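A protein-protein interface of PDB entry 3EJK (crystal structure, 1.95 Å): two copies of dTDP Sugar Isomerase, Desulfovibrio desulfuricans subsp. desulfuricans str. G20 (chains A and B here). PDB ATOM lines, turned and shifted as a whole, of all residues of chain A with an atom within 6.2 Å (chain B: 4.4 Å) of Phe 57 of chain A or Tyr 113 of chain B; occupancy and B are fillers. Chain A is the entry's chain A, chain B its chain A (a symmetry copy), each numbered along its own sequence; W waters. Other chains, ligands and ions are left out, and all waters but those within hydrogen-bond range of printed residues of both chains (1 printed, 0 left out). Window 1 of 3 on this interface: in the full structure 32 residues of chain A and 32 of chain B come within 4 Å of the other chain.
The backbone NH (N) of Met 41 of chain B sits close to the backbone carbonyl oxygen (O) of Ile 55 of chain A, 3.4 Å away. O of Phe 57 of chain A sits at hydrogen-bond distance from N of Leu 39 of chain B (2.8 Å). The backbone NH (N) of Glu 59 of chain A lies within hydrogen-bond range of the backbone carbonyl oxygen (O) of Pro 37 of chain B (3.0 Å). OE2 of Glu 59 of chain A is in salt-bridge range of NH2 of Arg 109 of chain B (3.0 Å).
The backbone carbonyl oxygen (O) of Tyr 56 of chain A is in hydrogen-bond range of the backbone NH (N) of Asn 138 of chain A, 2.9 Å away. O of Val 136 of chain A sits at hydrogen-bond distance from N of Ser 58 of chain A (2.8 Å). The backbone carbonyl oxygen (O) of His 40 of chain B is in hydrogen-bond range of the side-chain hydroxyl (OH) of Tyr 113 of chain B (2.8 Å). The backbone carbonyl oxygen of Ala 79 of chain B sits at hydrogen-bond distance from the backbone NH of Ala 137 of chain B (2.7 Å). The guanidinium group of Arg 109 of chain B lies within hydrogen-bond range of the backbone carbonyl oxygen of Pro 81 of chain B, 2.7 Å away. The backbone NH of Tyr 113 of chain B lies within hydrogen-bond range of the backbone carbonyl oxygen of Gly 108 of chain B (3.3 Å).
Val 38 of chain B touches Tyr 56 of chain A (CG1 to CD2, 3.9 Å). O of Phe 57 of chain A touches CA of Val 38 of chain B, at 3.3 Å. SD of Met 41 of chain B touches CZ of Phe 57 of chain A, 3.9 Å away. Phe 57 of chain A touches Phe 57 of chain B. Phe 57 of chain A touches Pro 81 of chain B. OH of Tyr 113 of chain B touches CD2 of Phe 57 of chain A (3.6 Å). CZ of Phe 57 of chain A touches CB of Ala 137 of chain B, 3.6 Å away. Ser 58 of chain A touches Pro 37 of chain B. CD2 of Leu 135 of chain A touches CG of Pro 81 of chain B (3.6 Å). Ala 137 of chain A touches Phe 57 of chain B (CB to CZ, 3.6 Å).
Phe 57 of chain A touches seven residues of chain B. Of the printed residues of chain B, Pro 81 of chain A touches Phe 57 (3.9 Å). Glu 27 of chain B touches none of the printed residues of chain A. Ala 79 of chain B touches none of the printed residues of chain A. Printed residues of chain A within 4 Å of Arg 109 of chain B: Glu 59. Tyr 113 of chain B touches just one residue of chain A: Phe 57 (3.6 Å). The nearest residue of chain B that does not touch Phe 57 of chain A is Pro 37 of chain B (4.2 Å). The nearest printed residue of chain A that does not touch Pro 37 of chain B is Phe 57 of chain A (4.2 Å).
Hydrophobic or aromatic side chains of chain B within 4 Å of the printed part of chain A: Pro 37, Val 38, Met 41, Phe 57, Pro 81, Tyr 113 and Ala 137. Of the 10 printed residues of chain A, 8 touch a printed residue of chain B. Hydrophobic or aromatic side chains of chain A within 4 Å of the printed part of chain B: Ile 55, Tyr 56, Phe 57, Pro 81, Leu 135 and Ala 137.
Phe 57 of chain B touches its own counterpart, Phe 57 of chain A. Phe 57 of chain A touches Pro 81 of chain B, and with the chains exchanged Pro 81 of chain A touches Phe 57 of chain B. Phe 57 of chain A touches Ala 137 of chain B, and with the chains exchanged Ala 137 of chain A touches Phe 57 of chain B. Positions printed for both chains: 57, 81 and 137. Of the 16 pairs that touch across the chains among the printed residues, 5 have their exchanged pair printed and touching as well.
Water W1 lies within hydrogen-bond range of O of Ile 55 of chain A and N of Met 41 of chain B.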
ATOM      1  N   ILE A  55      22.557 -31.818   9.005  1.00  0.00           N
ATOM      2  CA  ILE A  55      22.155 -31.115  10.228  1.00  0.00           C
ATOM      3  C   ILE A  55      21.430 -29.847   9.801  1.00  0.00           C
ATOM      4  O   ILE A  55      21.955 -29.040   9.016  1.00  0.00           O
ATOM      5  CB  ILE A  55      23.317 -30.753  11.184  1.00  0.00           C
ATOM      6  CG1 ILE A  55      22.787 -29.885  12.348  1.00  0.00           C
ATOM      7  CG2 ILE A  55      24.406 -30.010  10.478  1.00  0.00           C
ATOM      8  CD1 ILE A  55      21.892 -30.631  13.364  1.00  0.00           C
ATOM      9  N   TYR A  56      20.180 -29.743  10.253  1.00  0.00           N
ATOM     10  CA  TYR A  56      19.349 -28.553  10.045  1.00  0.00           C
ATOM     11  C   TYR A  56      18.526 -28.263  11.299  1.00  0.00           C
ATOM     12  O   TYR A  56      18.426 -29.078  12.210  1.00  0.00           O
ATOM     13  CB  TYR A  56      18.391 -28.692   8.846  1.00  0.00           C
ATOM     14  CG  TYR A  56      17.225 -29.631   9.058  1.00  0.00           C
ATOM     15  CD1 TYR A  56      17.346 -30.990   8.805  1.00  0.00           C
ATOM     16  CD2 TYR A  56      15.990 -29.158   9.521  1.00  0.00           C
ATOM     17  CE1 TYR A  56      16.268 -31.857   8.997  1.00  0.00           C
ATOM     18  CE2 TYR A  56      14.920 -30.022   9.731  1.00  0.00           C
ATOM     19  CZ  TYR A  56      15.070 -31.366   9.473  1.00  0.00           C
ATOM     20  OH  TYR A  56      14.022 -32.223   9.670  1.00  0.00           O
ATOM     21  N   PHE A  57      17.920 -27.093  11.272  1.00  0.00           N
ATOM     22  CA  PHE A  57      17.048 -26.615  12.338  1.00  0.00           C
ATOM     23  C   PHE A  57      15.674 -26.262  11.826  1.00  0.00           C
ATOM     24  O   PHE A  57      15.466 -25.931  10.648  1.00  0.00           O
ATOM     25  CB  PHE A  57      17.631 -25.377  13.008  1.00  0.00           C
ATOM     26  CG  PHE A  57      19.068 -25.503  13.308  1.00  0.00           C
ATOM     27  CD1 PHE A  57      19.494 -26.343  14.316  1.00  0.00           C
ATOM     28  CD2 PHE A  57      20.006 -24.812  12.562  1.00  0.00           C
ATOM     29  CE1 PHE A  57      20.839 -26.482  14.589  1.00  0.00           C
ATOM     30  CE2 PHE A  57      21.370 -24.936  12.839  1.00  0.00           C
ATOM     31  CZ  PHE A  57      21.783 -25.776  13.855  1.00  0.00           C
ATOM     32  N   SER A  58      14.749 -26.354  12.764  1.00  0.00           N
ATOM     33  CA  SER A  58      13.370 -26.031  12.520  1.00  0.00           C
ATOM     34  C   SER A  58      12.866 -25.148  13.638  1.00  0.00           C
ATOM     35  O   SER A  58      12.845 -25.539  14.806  1.00  0.00           O
ATOM     36  CB  SER A  58      12.528 -27.308  12.433  1.00  0.00           C
ATOM     37  OG  SER A  58      11.175 -27.031  12.157  1.00  0.00           O
ATOM     38  N   GLU A  59      12.473 -23.935  13.264  1.00  0.00           N
ATOM     39  CA  GLU A  59      11.901 -23.029  14.238  1.00  0.00           C
ATOM     40  C   GLU A  59      10.429 -23.317  14.319  1.00  0.00           C
ATOM     41  O   GLU A  59       9.779 -23.581  13.303  1.00  0.00           O
ATOM     42  CB  GLU A  59      12.132 -21.587  13.852  1.00  0.00           C
ATOM     43  CG  GLU A  59      11.446 -20.635  14.772  1.00  0.00           C
ATOM     44  CD  GLU A  59      11.964 -19.233  14.629  1.00  0.00           C
ATOM     45  OE1 GLU A  59      11.580 -18.522  13.685  1.00  0.00           O
ATOM     46  OE2 GLU A  59      12.741 -18.829  15.501  1.00  0.00           O
ATOM     47  N   PRO A  81      17.406 -27.323  21.750  1.00  0.00           N
ATOM     48  CA  PRO A  81      18.261 -26.484  22.604  1.00  0.00           C
ATOM     49  C   PRO A  81      17.661 -25.162  23.010  1.00  0.00           C
ATOM     50  O   PRO A  81      18.153 -24.511  23.931  1.00  0.00           O
ATOM     51  CB  PRO A  81      19.495 -26.240  21.745  1.00  0.00           C
ATOM     52  CG  PRO A  81      19.044 -26.457  20.344  1.00  0.00           C
ATOM     53  CD  PRO A  81      17.814 -27.298  20.345  1.00  0.00           C
ATOM     54  N   LEU A 135      13.449 -24.116  19.007  1.00  0.00           N
ATOM     55  CA  LEU A 135      14.400 -24.423  17.930  1.00  0.00           C
ATOM     56  C   LEU A 135      14.727 -25.892  18.039  1.00  0.00           C
ATOM     57  O   LEU A 135      15.335 -26.343  19.002  1.00  0.00           O
ATOM     58  CB  LEU A 135      15.698 -23.615  18.016  1.00  0.00           C
ATOM     59  CG  LEU A 135      16.541 -23.827  16.747  1.00  0.00           C
ATOM     60  CD1 LEU A 135      15.941 -22.993  15.571  1.00  0.00           C
ATOM     61  CD2 LEU A 135      17.981 -23.483  16.972  1.00  0.00           C
ATOM     62  N   VAL A 136      14.273 -26.628  17.046  1.00  0.00           N
ATOM     63  CA  VAL A 136      14.492 -28.054  16.972  1.00  0.00           C
ATOM     64  C   VAL A 136      15.684 -28.281  16.057  1.00  0.00           C
ATOM     65  O   VAL A 136      15.750 -27.724  14.969  1.00  0.00           O
ATOM     66  CB  VAL A 136      13.238 -28.772  16.367  1.00  0.00           C
ATOM     67  CG1 VAL A 136      13.419 -30.258  16.367  1.00  0.00           C
ATOM     68  CG2 VAL A 136      11.961 -28.379  17.125  1.00  0.00           C
ATOM     69  N   ALA A 137      16.633 -29.078  16.528  1.00  0.00           N
ATOM     70  CA  ALA A 137      17.777 -29.461  15.722  1.00  0.00           C
ATOM     71  C   ALA A 137      17.593 -30.908  15.327  1.00  0.00           C
ATOM     72  O   ALA A 137      17.127 -31.736  16.103  1.00  0.00           O
ATOM     73  CB  ALA A 137      19.093 -29.266  16.484  1.00  0.00           C
ATOM     74  N   ASN A 138      17.950 -31.204  14.090  1.00  0.00           N
ATOM     75  CA  ASN A 138      17.838 -32.566  13.586  1.00  0.00           C
ATOM     76  C   ASN A 138      19.097 -32.976  12.848  1.00  0.00           C
ATOM     77  O   ASN A 138      19.536 -32.296  11.941  1.00  0.00           O
ATOM     78  CB  ASN A 138      16.622 -32.689  12.659  1.00  0.00           C
ATOM     79  CG  ASN A 138      16.277 -34.125  12.334  1.00  0.00           C
ATOM     80  OD1 ASN A 138      16.872 -35.046  12.878  1.00  0.00           O
ATOM     81  ND2 ASN A 138      15.309 -34.323  11.438  1.00  0.00           N
ATOM     82  N   GLU B  27      26.797 -18.725   2.466  1.00  0.00           N
ATOM     83  CA  GLU B  27      25.341 -18.616   2.584  1.00  0.00           C
ATOM     84  C   GLU B  27      24.680 -19.879   3.061  1.00  0.00           C
ATOM     85  O   GLU B  27      25.053 -20.992   2.687  1.00  0.00           O
ATOM     86  CB  GLU B  27      24.700 -18.209   1.255  1.00  0.00           C
ATOM     87  CG  GLU B  27      24.905 -16.744   0.963  1.00  0.00           C
ATOM     88  CD  GLU B  27      24.391 -15.870   2.094  1.00  0.00           C
ATOM     89  OE1 GLU B  27      23.680 -16.392   3.006  1.00  0.00           O
ATOM     90  OE2 GLU B  27      24.710 -14.663   2.067  1.00  0.00           O
ATOM     91  N   LEU B  28      23.695 -19.660   3.919  1.00  0.00           N
ATOM     92  CA  LEU B  28      22.822 -20.706   4.450  1.00  0.00           C
ATOM     93  C   LEU B  28      21.369 -20.373   4.122  1.00  0.00           C
ATOM     94  O   LEU B  28      20.883 -19.274   4.410  1.00  0.00           O
ATOM     95  CB  LEU B  28      22.973 -20.856   5.970  1.00  0.00           C
ATOM     96  CG  LEU B  28      24.265 -21.449   6.502  1.00  0.00           C
ATOM     97  CD1 LEU B  28      24.283 -21.412   8.077  1.00  0.00           C
ATOM     98  CD2 LEU B  28      24.437 -22.854   5.950  1.00  0.00           C
ATOM     99  N   ARG B  29      20.671 -21.351   3.562  1.00  0.00           N
ATOM    100  CA  ARG B  29      19.282 -21.149   3.159  1.00  0.00           C
ATOM    101  C   ARG B  29      18.328 -21.216   4.324  1.00  0.00           C
ATOM    102  O   ARG B  29      18.482 -22.029   5.234  1.00  0.00           O
ATOM    103  CB  ARG B  29      18.841 -22.188   2.129  1.00  0.00           C
ATOM    104  CG  ARG B  29      17.788 -21.661   1.181  1.00  0.00           C
ATOM    105  CD  ARG B  29      17.154 -22.771   0.375  1.00  0.00           C
ATOM    106  NE  ARG B  29      18.139 -23.759  -0.053  1.00  0.00           N
ATOM    107  CZ  ARG B  29      17.817 -24.952  -0.545  1.00  0.00           C
ATOM    108  NH1 ARG B  29      16.536 -25.282  -0.666  1.00  0.00           N
ATOM    109  NH2 ARG B  29      18.765 -25.813  -0.905  1.00  0.00           N
ATOM    110  N   GLN B  30      17.357 -20.314   4.287  1.00  0.00           N
ATOM    111  CA  GLN B  30      16.225 -20.330   5.228  1.00  0.00           C
ATOM    112  C   GLN B  30      14.989 -20.665   4.395  1.00  0.00           C
ATOM    113  O   GLN B  30      14.606 -19.916   3.495  1.00  0.00           O
ATOM    114  CB  GLN B  30      16.045 -18.985   5.947  1.00  0.00           C
ATOM    115  CG  GLN B  30      17.308 -18.469   6.651  1.00  0.00           C
ATOM    116  CD  GLN B  30      17.138 -17.081   7.266  1.00  0.00           C
ATOM    117  OE1 GLN B  30      16.261 -16.846   8.100  1.00  0.00           O
ATOM    118  NE2 GLN B  30      17.989 -16.159   6.859  1.00  0.00           N
ATOM    119  N   PRO B  37      10.418 -21.079  10.023  1.00  0.00           N
ATOM    120  CA  PRO B  37      11.275 -21.562   8.966  1.00  0.00           C
ATOM    121  C   PRO B  37      12.201 -22.682   9.324  1.00  0.00           C
ATOM    122  O   PRO B  37      12.517 -22.928  10.488  1.00  0.00           O
ATOM    123  CB  PRO B  37      12.101 -20.316   8.610  1.00  0.00           C
ATOM    124  CG  PRO B  37      12.198 -19.569   9.901  1.00  0.00           C
ATOM    125  CD  PRO B  37      10.827 -19.747  10.503  1.00  0.00           C
ATOM    126  N   VAL B  38      12.604 -23.353   8.259  1.00  0.00           N
ATOM    127  CA  VAL B  38      13.633 -24.394   8.307  1.00  0.00           C
ATOM    128  C   VAL B  38      14.944 -23.703   7.956  1.00  0.00           C
ATOM    129  O   VAL B  38      15.054 -22.965   6.959  1.00  0.00           O
ATOM    130  CB  VAL B  38      13.334 -25.537   7.333  1.00  0.00           C
ATOM    131  CG1 VAL B  38      14.517 -26.455   7.191  1.00  0.00           C
ATOM    132  CG2 VAL B  38      12.069 -26.298   7.775  1.00  0.00           C
ATOM    133  N   LEU B  39      15.922 -23.925   8.812  1.00  0.00           N
ATOM    134  CA  LEU B  39      17.227 -23.318   8.668  1.00  0.00           C
ATOM    135  C   LEU B  39      18.295 -24.352   8.393  1.00  0.00           C
ATOM    136  O   LEU B  39      18.560 -25.229   9.212  1.00  0.00           O
ATOM    137  CB  LEU B  39      17.572 -22.553   9.936  1.00  0.00           C
ATOM    138  CG  LEU B  39      16.473 -21.626  10.454  1.00  0.00           C
ATOM    139  CD1 LEU B  39      16.831 -21.073  11.818  1.00  0.00           C
ATOM    140  CD2 LEU B  39      16.241 -20.518   9.424  1.00  0.00           C
ATOM    141  N   HIS B  40      18.917 -24.236   7.230  1.00  0.00           N
ATOM    142  CA  HIS B  40      19.993 -25.163   6.895  1.00  0.00           C
ATOM    143  C   HIS B  40      21.276 -24.858   7.632  1.00  0.00           C
ATOM    144  O   HIS B  40      21.495 -23.769   8.144  1.00  0.00           O
ATOM    145  CB  HIS B  40      20.316 -25.219   5.405  1.00  0.00           C
ATOM    146  CG  HIS B  40      19.258 -25.891   4.596  1.00  0.00           C
ATOM    147  ND1 HIS B  40      19.243 -25.866   3.222  1.00  0.00           N
ATOM    148  CD2 HIS B  40      18.142 -26.556   4.972  1.00  0.00           C
ATOM    149  CE1 HIS B  40      18.198 -26.545   2.781  1.00  0.00           C
ATOM    150  NE2 HIS B  40      17.500 -26.956   3.825  1.00  0.00           N
ATOM    151  N   MET B  41      22.112 -25.878   7.666  1.00  0.00           N
ATOM    152  CA  MET B  41      23.449 -25.748   8.213  1.00  0.00           C
ATOM    153  C   MET B  41      24.500 -26.477   7.368  1.00  0.00           C
ATOM    154  O   MET B  41      25.399 -25.856   6.774  1.00  0.00           O
ATOM    155  CB  MET B  41      23.533 -26.228   9.659  1.00  0.00           C
ATOM    156  CG  MET B  41      24.871 -25.866  10.231  1.00  0.00           C
ATOM    157  SD  MET B  41      25.142 -26.373  12.062  1.00  0.00           S
ATOM    158  CE  MET B  41      26.993 -25.645  12.330  1.00  0.00           C
ATOM    159  N   PHE B  57      26.084 -27.139  20.722  1.00  0.00           N
ATOM    160  CA  PHE B  57      25.609 -25.764  20.828  1.00  0.00           C
ATOM    161  C   PHE B  57      26.208 -25.052  22.014  1.00  0.00           C
ATOM    162  O   PHE B  57      26.615 -25.655  23.019  1.00  0.00           O
ATOM    163  CB  PHE B  57      24.093 -25.718  20.970  1.00  0.00           C
ATOM    164  CG  PHE B  57      23.395 -26.609  20.027  1.00  0.00           C
ATOM    165  CD1 PHE B  57      23.355 -26.300  18.683  1.00  0.00           C
ATOM    166  CD2 PHE B  57      22.806 -27.780  20.470  1.00  0.00           C
ATOM    167  CE1 PHE B  57      22.721 -27.140  17.791  1.00  0.00           C
ATOM    168  CE2 PHE B  57      22.150 -28.631  19.576  1.00  0.00           C
ATOM    169  CZ  PHE B  57      22.111 -28.307  18.233  1.00  0.00           C
ATOM    170  N   ALA B  79      27.207 -21.717  13.018  1.00  0.00           N
ATOM    171  CA  ALA B  79      25.932 -21.154  12.540  1.00  0.00           C
ATOM    172  C   ALA B  79      25.210 -20.628  13.766  1.00  0.00           C
ATOM    173  O   ALA B  79      25.398 -21.140  14.855  1.00  0.00           O
ATOM    174  CB  ALA B  79      25.075 -22.145  11.749  1.00  0.00           C
ATOM    175  N   VAL B  80      24.442 -19.558  13.581  1.00  0.00           N
ATOM    176  CA  VAL B  80      23.730 -18.906  14.692  1.00  0.00           C
ATOM    177  C   VAL B  80      22.226 -18.823  14.377  1.00  0.00           C
ATOM    178  O   VAL B  80      21.728 -17.813  13.870  1.00  0.00           O
ATOM    179  CB  VAL B  80      24.315 -17.508  14.978  1.00  0.00           C
ATOM    180  CG1 VAL B  80      23.537 -16.821  16.087  1.00  0.00           C
ATOM    181  CG2 VAL B  80      25.839 -17.620  15.368  1.00  0.00           C
ATOM    182  N   PRO B  81      21.493 -19.886  14.688  1.00  0.00           N
ATOM    183  CA  PRO B  81      20.067 -19.938  14.331  1.00  0.00           C
ATOM    184  C   PRO B  81      19.148 -19.170  15.247  1.00  0.00           C
ATOM    185  O   PRO B  81      17.995 -18.913  14.901  1.00  0.00           O
ATOM    186  CB  PRO B  81      19.734 -21.423  14.405  1.00  0.00           C
ATOM    187  CG  PRO B  81      20.769 -22.010  15.297  1.00  0.00           C
ATOM    188  CD  PRO B  81      21.960 -21.114  15.331  1.00  0.00           C
ATOM    189  N   GLY B 108      23.879 -14.241  12.477  1.00  0.00           N
ATOM    190  CA  GLY B 108      22.485 -14.273  12.942  1.00  0.00           C
ATOM    191  C   GLY B 108      21.460 -13.752  11.959  1.00  0.00           C
ATOM    192  O   GLY B 108      21.749 -13.004  11.032  1.00  0.00           O
ATOM    193  N   ARG B 109      20.245 -14.210  12.197  1.00  0.00           N
ATOM    194  CA  ARG B 109      19.065 -13.851  11.421  1.00  0.00           C
ATOM    195  C   ARG B 109      18.629 -12.427  11.710  1.00  0.00           C
ATOM    196  O   ARG B 109      18.828 -11.934  12.807  1.00  0.00           O
ATOM    197  CB  ARG B 109      17.912 -14.819  11.717  1.00  0.00           C
ATOM    198  CG  ARG B 109      18.186 -16.206  11.219  1.00  0.00           C
ATOM    199  CD  ARG B 109      16.896 -17.013  11.250  1.00  0.00           C
ATOM    200  NE  ARG B 109      16.659 -17.531  12.568  1.00  0.00           N
ATOM    201  CZ  ARG B 109      15.473 -17.812  13.081  1.00  0.00           C
ATOM    202  NH1 ARG B 109      14.358 -17.564  12.419  1.00  0.00           N
ATOM    203  NH2 ARG B 109      15.425 -18.310  14.291  1.00  0.00           N
ATOM    204  N   ASP B 111      19.464 -11.285   8.484  1.00  0.00           N
ATOM    205  CA  ASP B 111      20.281 -10.875   7.357  1.00  0.00           C
ATOM    206  C   ASP B 111      21.701 -11.369   7.379  1.00  0.00           C
ATOM    207  O   ASP B 111      22.452 -11.138   6.438  1.00  0.00           O
ATOM    208  CB  ASP B 111      20.297  -9.351   7.242  1.00  0.00           C
ATOM    209  CG  ASP B 111      18.911  -8.764   7.019  1.00  0.00           C
ATOM    210  OD1 ASP B 111      18.054  -9.474   6.465  1.00  0.00           O
ATOM    211  OD2 ASP B 111      18.706  -7.578   7.371  1.00  0.00           O
ATOM    212  N   ASN B 112      22.058 -12.065   8.441  1.00  0.00           N
ATOM    213  CA  ASN B 112      23.418 -12.556   8.586  1.00  0.00           C
ATOM    214  C   ASN B 112      23.511 -14.029   8.895  1.00  0.00           C
ATOM    215  O   ASN B 112      24.404 -14.470   9.633  1.00  0.00           O
ATOM    216  CB  ASN B 112      24.116 -11.763   9.672  1.00  0.00           C
ATOM    217  CG  ASN B 112      24.465 -10.351   9.221  1.00  0.00           C
ATOM    218  OD1 ASN B 112      25.281 -10.155   8.331  1.00  0.00           O
ATOM    219  ND2 ASN B 112      23.844  -9.374   9.833  1.00  0.00           N
ATOM    220  N   TYR B 113      22.549 -14.776   8.381  1.00  0.00           N
ATOM    221  CA  TYR B 113      22.507 -16.235   8.614  1.00  0.00           C
ATOM    222  C   TYR B 113      23.445 -16.955   7.630  1.00  0.00           C
ATOM    223  O   TYR B 113      23.090 -17.304   6.510  1.00  0.00           O
ATOM    224  CB  TYR B 113      21.083 -16.770   8.581  1.00  0.00           C
ATOM    225  CG  TYR B 113      21.043 -18.204   9.050  1.00  0.00           C
ATOM    226  CD1 TYR B 113      21.398 -18.521  10.350  1.00  0.00           C
ATOM    227  CD2 TYR B 113      20.667 -19.237   8.197  1.00  0.00           C
ATOM    228  CE1 TYR B 113      21.377 -19.817  10.798  1.00  0.00           C
ATOM    229  CE2 TYR B 113      20.647 -20.542   8.626  1.00  0.00           C
ATOM    230  CZ  TYR B 113      21.000 -20.830   9.937  1.00  0.00           C
ATOM    231  OH  TYR B 113      21.016 -22.130  10.379  1.00  0.00           O
ATOM    232  N   ARG B 114      24.681 -17.100   8.079  1.00  0.00           N
ATOM    233  CA  ARG B 114      25.756 -17.718   7.305  1.00  0.00           C
ATOM    234  C   ARG B 114      26.544 -18.711   8.112  1.00  0.00           C
ATOM    235  O   ARG B 114      26.415 -18.808   9.347  1.00  0.00           O
ATOM    236  CB  ARG B 114      26.703 -16.645   6.819  1.00  0.00           C
ATOM    237  CG  ARG B 114      25.961 -15.540   6.054  1.00  0.00           C
ATOM    238  CD  ARG B 114      26.879 -14.431   5.633  1.00  0.00           C
ATOM    239  NE  ARG B 114      26.218 -13.532   4.688  1.00  0.00           N
ATOM    240  CZ  ARG B 114      25.779 -12.307   4.975  1.00  0.00           C
ATOM    241  NH1 ARG B 114      25.940 -11.805   6.186  1.00  0.00           N
ATOM    242  NH2 ARG B 114      25.188 -11.572   4.036  1.00  0.00           N
ATOM    243  N   ALA B 137      25.655 -22.794  16.959  1.00  0.00           N
ATOM    244  CA  ALA B 137      25.811 -24.199  16.633  1.00  0.00           C
ATOM    245  C   ALA B 137      27.173 -24.373  16.003  1.00  0.00           C
ATOM    246  O   ALA B 137      27.637 -23.544  15.228  1.00  0.00           O
ATOM    247  CB  ALA B 137      24.705 -24.684  15.688  1.00  0.00           C
HETATM  248  O   HOH W   1      21.118 -28.336   6.188  1.00  0.00           O
